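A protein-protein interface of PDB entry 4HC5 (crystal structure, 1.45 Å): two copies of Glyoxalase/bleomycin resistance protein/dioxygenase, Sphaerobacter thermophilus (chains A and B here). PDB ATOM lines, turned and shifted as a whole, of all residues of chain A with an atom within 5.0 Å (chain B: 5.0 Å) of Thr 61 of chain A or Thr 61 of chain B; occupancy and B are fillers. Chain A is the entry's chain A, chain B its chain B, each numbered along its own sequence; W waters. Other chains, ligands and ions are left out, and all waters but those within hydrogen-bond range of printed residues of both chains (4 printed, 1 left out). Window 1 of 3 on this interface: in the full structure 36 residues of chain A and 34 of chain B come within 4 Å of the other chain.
The side-chain hydroxyl (OG1) of Thr 61 of chain A is in hydrogen-bond range of the side-chain hydroxyl (OG1) of Thr 61 of chain B, 3.2 Å away.
The backbone carbonyl oxygen (O) of Val 14 of chain A sits at hydrogen-bond distance from the side-chain hydroxyl (OG1) of Thr 61 of chain A.
The backbone NH (N) of Ala 17 of chain A is in hydrogen-bond range of the backbone carbonyl oxygen (O) of Gln 62 of chain A (3.2 Å).
O of Val 54 of chain A sits at hydrogen-bond distance from N of Val 63 of chain A.
OG1 of Thr 61 of chain B is in hydrogen-bond range of O of Val 14 of chain B (2.6 Å).
The backbone NH (N) of Ala 17 of chain B is in hydrogen-bond range of the backbone carbonyl oxygen (O) of Gln 62 of chain B.
N of Val 63 of chain B sits at hydrogen-bond distance from O of Val 54 of chain B (2.9 Å).
Among the printed residues, merely in contact across the chains: Val 14 of chain A with Val 63 of chain B (3.99 Å), Ala 17 of chain A with Ala 17 of chain B (3.8 Å), Gln 60 of chain A with Gln 60 of chain B (3.8 Å), Thr 61 of chain A with Val 14 of chain B (3.97 Å) and Val 63 of chain A with Val 14 of chain B (3.9 Å).
Water W2 lies within hydrogen-bond range of the side-chain amide oxygen (OE1) of Gln 60 of chain A (2.6 Å), the side-chain hydroxyl (OG1) of Thr 61 of chain A (2.7 Å), the backbone NH (N) of Thr 61 of chain B (2.9 Å) and the backbone NH (N) of Gln 60 of chain B (3.4 Å).
Water W3 lies within hydrogen-bond range of OE1 of Gln 60 of chain B, OG1 of Thr 61 of chain B, N of Thr 61 of chain A and N of Gln 60 of chain A.
Water W4 lies within hydrogen-bond range of the backbone carbonyl oxygen of Thr 61 of chain A (2.8 Å) and the backbone NH of Val 14 of chain B (2.8 Å).
Water W1 bridges O of Thr 61 of chain B (2.8 Å) and N of Val 14 of chain A (2.9 Å).
Thr 61 of chain A touches two residues of chain B.
Printed residues of chain A within 4 Å of Thr 61 of chain B: Thr 61 (3.2 Å).
Of the printed residues of chain B, Gln 60 of chain A touches Gln 60 (3.8 Å).
Of the printed residues of chain A, Gln 60 of chain B touches Gln 60 (3.8 Å).
Of the printed residues of chain A, Val 63 of chain B touches Val 14.
Of the printed residues of chain B, Ala 17 of chain A touches Ala 17 (3.8 Å).
Of the printed residues of chain A, Val 14 of chain B touches Thr 61 (3.97 Å) and Val 63 (3.9 Å).
Ser 16 of chain A touches none of the printed residues of chain B.
Pro 56 of chain B touches none of the printed residues of chain A.
The nearest printed residue of chain B that does not touch Thr 61 of chain A is Gln 60 of chain B (5.2 Å).
The nearest printed residue of chain A that does not touch Thr 61 of chain B is Val 14 of chain A (4.01 Å).
The nearest printed residue of chain B that does not touch Val 14 of chain A is Thr 61 of chain B (4.01 Å).
Of the 12 printed residues of chain A, 5 touch a printed residue of chain B.
Of the 12 printed residues of chain B, 5 touch a printed residue of chain A.
Printed residues of chain B that touch a printed residue of chain A: Val 14, Ala 17, Gln 60, Thr 61 and Val 63.
Hydrophobic or aromatic side chains of chain B that line the printed part of chain A: Val 14, Ala 17 and Val 63.
Among the printed residues, 6 pairs touch across the chains.
Among the printed residues, no Asp or Glu carboxylate lies within 4 Å of a Lys or Arg side-chain nitrogen of the other chain.
Val 14 of chain A touches Val 63 of chain B, and with the chains exchanged Val 63 of chain A touches Val 14 of chain B.
Ala 17 of chain A touches its own counterpart, Ala 17 of chain B.
Gln 60 of chain A touches its own counterpart, Gln 60 of chain B.
Thr 61 of chain B touches its own counterpart, Thr 61 of chain A.
Of the 6 pairs that touch across the chains among the printed residues, 5 have their exchanged pair printed and touching as well.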
ATOM      1  N   VAL A  14     -15.348  -3.289   4.767  1.00  0.00           N
ATOM      2  CA  VAL A  14     -16.348  -3.694   3.765  1.00  0.00           C
ATOM      3  C   VAL A  14     -17.535  -4.340   4.494  1.00  0.00           C
ATOM      4  O   VAL A  14     -17.395  -5.359   5.158  1.00  0.00           O
ATOM      5  CB  VAL A  14     -15.761  -4.617   2.738  1.00  0.00           C
ATOM      6  CG1 VAL A  14     -16.903  -5.063   1.768  1.00  0.00           C
ATOM      7  CG2 VAL A  14     -14.587  -3.975   1.992  1.00  0.00           C
ATOM      8  N   HIS A  15     -18.713  -3.719   4.409  1.00  0.00           N
ATOM      9  CA  HIS A  15     -19.904  -4.280   5.032  1.00  0.00           C
ATOM     10  C   HIS A  15     -20.352  -5.591   4.359  1.00  0.00           C
ATOM     11  O   HIS A  15     -20.653  -6.590   5.032  1.00  0.00           O
ATOM     12  CB  HIS A  15     -21.063  -3.267   4.993  1.00  0.00           C
ATOM     13  CG  HIS A  15     -22.288  -3.822   5.585  1.00  0.00           C
ATOM     14  ND1 HIS A  15     -23.197  -4.556   4.856  1.00  0.00           N
ATOM     15  CD2 HIS A  15     -22.726  -3.841   6.872  1.00  0.00           C
ATOM     16  CE1 HIS A  15     -24.168  -5.001   5.703  1.00  0.00           C
ATOM     17  NE2 HIS A  15     -23.876  -4.581   6.927  1.00  0.00           N
ATOM     18  N   SER A  16     -20.408  -5.542   3.042  1.00  0.00           N
ATOM     19  CA  SER A  16     -21.011  -6.633   2.260  1.00  0.00           C
ATOM     20  C   SER A  16     -20.641  -6.451   0.798  1.00  0.00           C
ATOM     21  O   SER A  16     -20.396  -5.371   0.335  1.00  0.00           O
ATOM     22  CB  SER A  16     -22.526  -6.682   2.399  1.00  0.00           C
ATOM     23  OG  SER A  16     -23.151  -5.436   2.246  1.00  0.00           O
ATOM     24  N   ALA A  17     -20.646  -7.602   0.108  1.00  0.00           N
ATOM     25  CA  ALA A  17     -20.647  -7.681  -1.364  1.00  0.00           C
ATOM     26  C   ALA A  17     -21.936  -8.445  -1.753  1.00  0.00           C
ATOM     27  O   ALA A  17     -22.561  -9.069  -0.902  1.00  0.00           O
ATOM     28  CB  ALA A  17     -19.415  -8.428  -1.836  1.00  0.00           C
ATOM     29  N   VAL A  54     -26.214 -12.914   4.370  1.00  0.00           N
ATOM     30  CA  VAL A  54     -25.702 -14.058   5.080  1.00  0.00           C
ATOM     31  C   VAL A  54     -24.193 -13.824   5.373  1.00  0.00           C
ATOM     32  O   VAL A  54     -23.516 -13.065   4.712  1.00  0.00           O
ATOM     33  CB  VAL A  54     -25.870 -15.388   4.275  1.00  0.00           C
ATOM     34  CG1 VAL A  54     -27.339 -15.802   4.230  1.00  0.00           C
ATOM     35  CG2 VAL A  54     -25.280 -15.273   2.862  1.00  0.00           C
ATOM     36  N   VAL A  55     -23.712 -14.482   6.439  1.00  0.00           N
ATOM     37  CA  VAL A  55     -22.319 -14.279   6.842  1.00  0.00           C
ATOM     38  C   VAL A  55     -21.713 -15.617   7.303  1.00  0.00           C
ATOM     39  O   VAL A  55     -22.371 -16.380   7.956  1.00  0.00           O
ATOM     40  CB  VAL A  55     -22.195 -13.224   7.993  1.00  0.00           C
ATOM     41  CG1 VAL A  55     -22.747 -13.733   9.335  1.00  0.00           C
ATOM     42  CG2 VAL A  55     -20.777 -12.710   8.166  1.00  0.00           C
ATOM     43  N   PRO A  56     -20.431 -15.852   6.982  1.00  0.00           N
ATOM     44  CA  PRO A  56     -19.787 -16.984   7.626  1.00  0.00           C
ATOM     45  C   PRO A  56     -19.744 -16.798   9.126  1.00  0.00           C
ATOM     46  O   PRO A  56     -19.548 -15.677   9.598  1.00  0.00           O
ATOM     47  CB  PRO A  56     -18.356 -16.995   7.004  1.00  0.00           C
ATOM     48  CG  PRO A  56     -18.536 -16.279   5.677  1.00  0.00           C
ATOM     49  CD  PRO A  56     -19.558 -15.187   6.003  1.00  0.00           C
ATOM     50  N   ALA A  59     -17.588 -14.078  11.228  1.00  0.00           N
ATOM     51  CA  ALA A  59     -16.892 -13.199  10.297  1.00  0.00           C
ATOM     52  C   ALA A  59     -17.521 -11.837  10.190  1.00  0.00           C
ATOM     53  O   ALA A  59     -18.711 -11.656  10.540  1.00  0.00           O
ATOM     54  CB  ALA A  59     -16.796 -13.854   8.908  1.00  0.00           C
ATOM     55  N   GLN A  60     -16.738 -10.890   9.676  1.00  0.00           N
ATOM     56  CA  GLN A  60     -17.220  -9.474   9.574  1.00  0.00           C
ATOM     57  C   GLN A  60     -18.104  -9.194   8.310  1.00  0.00           C
ATOM     58  O   GLN A  60     -19.282  -8.827   8.396  1.00  0.00           O
ATOM     59  CB  GLN A  60     -16.064  -8.566   9.679  1.00  0.00           C
ATOM     60  CG  GLN A  60     -16.358  -7.112   9.581  1.00  0.00           C
ATOM     61  CD  GLN A  60     -15.105  -6.285   9.805  1.00  0.00           C
ATOM     62  OE1 GLN A  60     -14.087  -6.404   9.106  1.00  0.00           O
ATOM     63  NE2 GLN A  60     -15.152  -5.485  10.898  1.00  0.00           N
ATOM     64  N   THR A  61     -17.550  -9.435   7.152  1.00  0.00           N
ATOM     65  CA  THR A  61     -18.150  -9.059   5.872  1.00  0.00           C
ATOM     66  C   THR A  61     -19.254 -10.087   5.483  1.00  0.00           C
ATOM     67  O   THR A  61     -18.993 -11.290   5.407  1.00  0.00           O
ATOM     68  CB  THR A  61     -17.092  -8.853   4.825  1.00  0.00           C
ATOM     69  OG1 THR A  61     -16.182  -7.842   5.218  1.00  0.00           O
ATOM     70  CG2 THR A  61     -17.697  -8.493   3.462  1.00  0.00           C
ATOM     71  N   GLN A  62     -20.391  -9.559   5.116  1.00  0.00           N
ATOM     72  CA  GLN A  62     -21.591 -10.308   4.710  1.00  0.00           C
ATOM     73  C   GLN A  62     -21.655 -10.433   3.192  1.00  0.00           C
ATOM     74  O   GLN A  62     -20.968  -9.701   2.460  1.00  0.00           O
ATOM     75  CB  GLN A  62     -22.799  -9.593   5.261  1.00  0.00           C
ATOM     76  CG  GLN A  62     -22.844  -9.457   6.774  1.00  0.00           C
ATOM     77  CD  GLN A  62     -23.940  -8.531   7.287  1.00  0.00           C
ATOM     78  OE1 GLN A  62     -24.944  -8.266   6.607  1.00  0.00           O
ATOM     79  NE2 GLN A  62     -23.727  -8.000   8.495  1.00  0.00           N
ATOM     80  N   VAL A  63     -22.496 -11.339   2.724  1.00  0.00           N
ATOM     81  CA  VAL A  63     -22.851 -11.454   1.305  1.00  0.00           C
ATOM     82  C   VAL A  63     -24.373 -11.207   1.198  1.00  0.00           C
ATOM     83  O   VAL A  63     -25.177 -11.870   1.877  1.00  0.00           O
ATOM     84  CB  VAL A  63     -22.506 -12.862   0.776  1.00  0.00           C
ATOM     85  CG1 VAL A  63     -23.002 -13.061  -0.687  1.00  0.00           C
ATOM     86  CG2 VAL A  63     -20.990 -13.136   0.937  1.00  0.00           C
ATOM     87  N   VAL B  14     -15.072 -14.354   4.034  1.00  0.00           N
ATOM     88  CA  VAL B  14     -14.876 -13.842   2.676  1.00  0.00           C
ATOM     89  C   VAL B  14     -13.499 -13.196   2.521  1.00  0.00           C
ATOM     90  O   VAL B  14     -13.155 -12.220   3.254  1.00  0.00           O
ATOM     91  CB  VAL B  14     -15.955 -12.791   2.270  1.00  0.00           C
ATOM     92  CG1 VAL B  14     -15.676 -12.252   0.866  1.00  0.00           C
ATOM     93  CG2 VAL B  14     -17.383 -13.386   2.442  1.00  0.00           C
ATOM     94  N   HIS B  15     -12.673 -13.720   1.624  1.00  0.00           N
ATOM     95  CA  HIS B  15     -11.321 -13.202   1.473  1.00  0.00           C
ATOM     96  C   HIS B  15     -11.314 -11.862   0.813  1.00  0.00           C
ATOM     97  O   HIS B  15     -10.609 -10.925   1.245  1.00  0.00           O
ATOM     98  CB  HIS B  15     -10.470 -14.155   0.649  1.00  0.00           C
ATOM     99  CG  HIS B  15      -9.077 -13.642   0.369  1.00  0.00           C
ATOM    100  ND1 HIS B  15      -8.781 -12.912  -0.720  1.00  0.00           N
ATOM    101  CD2 HIS B  15      -7.890 -13.782   1.084  1.00  0.00           C
ATOM    102  CE1 HIS B  15      -7.472 -12.597  -0.707  1.00  0.00           C
ATOM    103  NE2 HIS B  15      -6.928 -13.131   0.399  1.00  0.00           N
ATOM    104  N   SER B  16     -12.095 -11.763  -0.251  1.00  0.00           N
ATOM    105  CA  SER B  16     -12.100 -10.624  -1.119  1.00  0.00           C
ATOM    106  C   SER B  16     -13.278 -10.675  -2.071  1.00  0.00           C
ATOM    107  O   SER B  16     -13.784 -11.721  -2.405  1.00  0.00           O
ATOM    108  CB  SER B  16     -10.809 -10.503  -1.949  1.00  0.00           C
ATOM    109  OG  SER B  16     -10.467 -11.701  -2.594  1.00  0.00           O
ATOM    110  N   ALA B  17     -13.652  -9.473  -2.498  1.00  0.00           N
ATOM    111  CA  ALA B  17     -14.555  -9.221  -3.630  1.00  0.00           C
ATOM    112  C   ALA B  17     -13.823  -8.412  -4.649  1.00  0.00           C
ATOM    113  O   ALA B  17     -12.834  -7.783  -4.340  1.00  0.00           O
ATOM    114  CB  ALA B  17     -15.841  -8.497  -3.138  1.00  0.00           C
ATOM    115  N   VAL B  54      -6.562  -4.308  -2.128  1.00  0.00           N
ATOM    116  CA  VAL B  54      -6.540  -3.265  -1.128  1.00  0.00           C
ATOM    117  C   VAL B  54      -7.470  -3.609   0.017  1.00  0.00           C
ATOM    118  O   VAL B  54      -8.468  -4.264  -0.141  1.00  0.00           O
ATOM    119  CB  VAL B  54      -6.858  -1.866  -1.687  1.00  0.00           C
ATOM    120  CG1 VAL B  54      -5.677  -1.384  -2.595  1.00  0.00           C
ATOM    121  CG2 VAL B  54      -8.165  -1.817  -2.511  1.00  0.00           C
ATOM    122  N   VAL B  55      -7.190  -3.070   1.224  1.00  0.00           N
ATOM    123  CA  VAL B  55      -8.007  -3.346   2.387  1.00  0.00           C
ATOM    124  C   VAL B  55      -8.171  -2.087   3.246  1.00  0.00           C
ATOM    125  O   VAL B  55      -7.211  -1.322   3.395  1.00  0.00           O
ATOM    126  CB  VAL B  55      -7.409  -4.517   3.246  1.00  0.00           C
ATOM    127  CG1 VAL B  55      -6.085  -4.099   3.944  1.00  0.00           C
ATOM    128  CG2 VAL B  55      -8.429  -5.093   4.203  1.00  0.00           C
ATOM    129  N   PRO B  56      -9.322  -1.870   3.822  1.00  0.00           N
ATOM    130  CA  PRO B  56      -9.402  -0.799   4.826  1.00  0.00           C
ATOM    131  C   PRO B  56      -8.473  -1.176   6.029  1.00  0.00           C
ATOM    132  O   PRO B  56      -8.434  -2.336   6.449  1.00  0.00           O
ATOM    133  CB  PRO B  56     -10.875  -0.821   5.247  1.00  0.00           C
ATOM    134  CG  PRO B  56     -11.583  -1.382   4.051  1.00  0.00           C
ATOM    135  CD  PRO B  56     -10.642  -2.483   3.574  1.00  0.00           C
ATOM    136  N   ALA B  59      -8.917  -4.158   8.730  1.00  0.00           N
ATOM    137  CA  ALA B  59     -10.084  -4.968   8.348  1.00  0.00           C
ATOM    138  C   ALA B  59      -9.651  -6.301   7.726  1.00  0.00           C
ATOM    139  O   ALA B  59      -8.557  -6.448   7.229  1.00  0.00           O
ATOM    140  CB  ALA B  59     -11.011  -4.192   7.404  1.00  0.00           C
ATOM    141  N   GLN B  60     -10.622  -7.223   7.674  1.00  0.00           N
ATOM    142  CA  GLN B  60     -10.345  -8.572   7.150  1.00  0.00           C
ATOM    143  C   GLN B  60     -10.500  -8.698   5.633  1.00  0.00           C
ATOM    144  O   GLN B  60      -9.599  -9.088   4.959  1.00  0.00           O
ATOM    145  CB  GLN B  60     -11.259  -9.552   7.854  1.00  0.00           C
ATOM    146  CG  GLN B  60     -10.983 -10.983   7.476  1.00  0.00           C
ATOM    147  CD  GLN B  60     -11.799 -11.914   8.307  1.00  0.00           C
ATOM    148  OE1 GLN B  60     -13.046 -11.804   8.388  1.00  0.00           O
ATOM    149  NE2 GLN B  60     -11.118 -12.847   8.953  1.00  0.00           N
ATOM    150  N   THR B  61     -11.674  -8.377   5.117  1.00  0.00           N
ATOM    151  CA  THR B  61     -11.959  -8.649   3.683  1.00  0.00           C
ATOM    152  C   THR B  61     -11.369  -7.572   2.813  1.00  0.00           C
ATOM    153  O   THR B  61     -11.539  -6.357   3.034  1.00  0.00           O
ATOM    154  CB  THR B  61     -13.454  -8.832   3.532  1.00  0.00           C
ATOM    155  OG1 THR B  61     -13.953  -9.920   4.297  1.00  0.00           O
ATOM    156  CG2 THR B  61     -13.822  -8.963   2.042  1.00  0.00           C
ATOM    157  N   GLN B  62     -10.734  -7.999   1.772  1.00  0.00           N
ATOM    158  CA  GLN B  62     -10.098  -7.165   0.790  1.00  0.00           C
ATOM    159  C   GLN B  62     -10.993  -6.899  -0.430  1.00  0.00           C
ATOM    160  O   GLN B  62     -11.968  -7.585  -0.692  1.00  0.00           O
ATOM    161  CB  GLN B  62      -8.761  -7.805   0.378  1.00  0.00           C
ATOM    162  CG  GLN B  62      -7.773  -8.088   1.538  1.00  0.00           C
ATOM    163  CD  GLN B  62      -6.675  -9.041   1.163  1.00  0.00           C
ATOM    164  OE1 GLN B  62      -6.247  -9.181  -0.035  1.00  0.00           O
ATOM    165  NE2 GLN B  62      -6.137  -9.630   2.213  1.00  0.00           N
ATOM    166  N   VAL B  63     -10.553  -5.908  -1.195  1.00  0.00           N
ATOM    167  CA  VAL B  63     -11.085  -5.583  -2.532  1.00  0.00           C
ATOM    168  C   VAL B  63     -10.003  -5.788  -3.595  1.00  0.00           C
ATOM    169  O   VAL B  63      -8.949  -5.156  -3.523  1.00  0.00           O
ATOM    170  CB  VAL B  63     -11.689  -4.174  -2.645  1.00  0.00           C
ATOM    171  CG1 VAL B  63     -12.238  -3.842  -4.027  1.00  0.00           C
ATOM    172  CG2 VAL B  63     -12.753  -3.963  -1.550  1.00  0.00           C
HETATM  173  O   HOH W   1     -13.172  -5.149   5.022  1.00  0.00           O
HETATM  174  O   HOH W   2     -13.913  -7.301   6.654  1.00  0.00           O
HETATM  175  O   HOH W   3     -14.851 -10.633   6.767  1.00  0.00           O
HETATM  176  O   HOH W   4     -16.564 -12.625   5.736  1.00  0.00           O
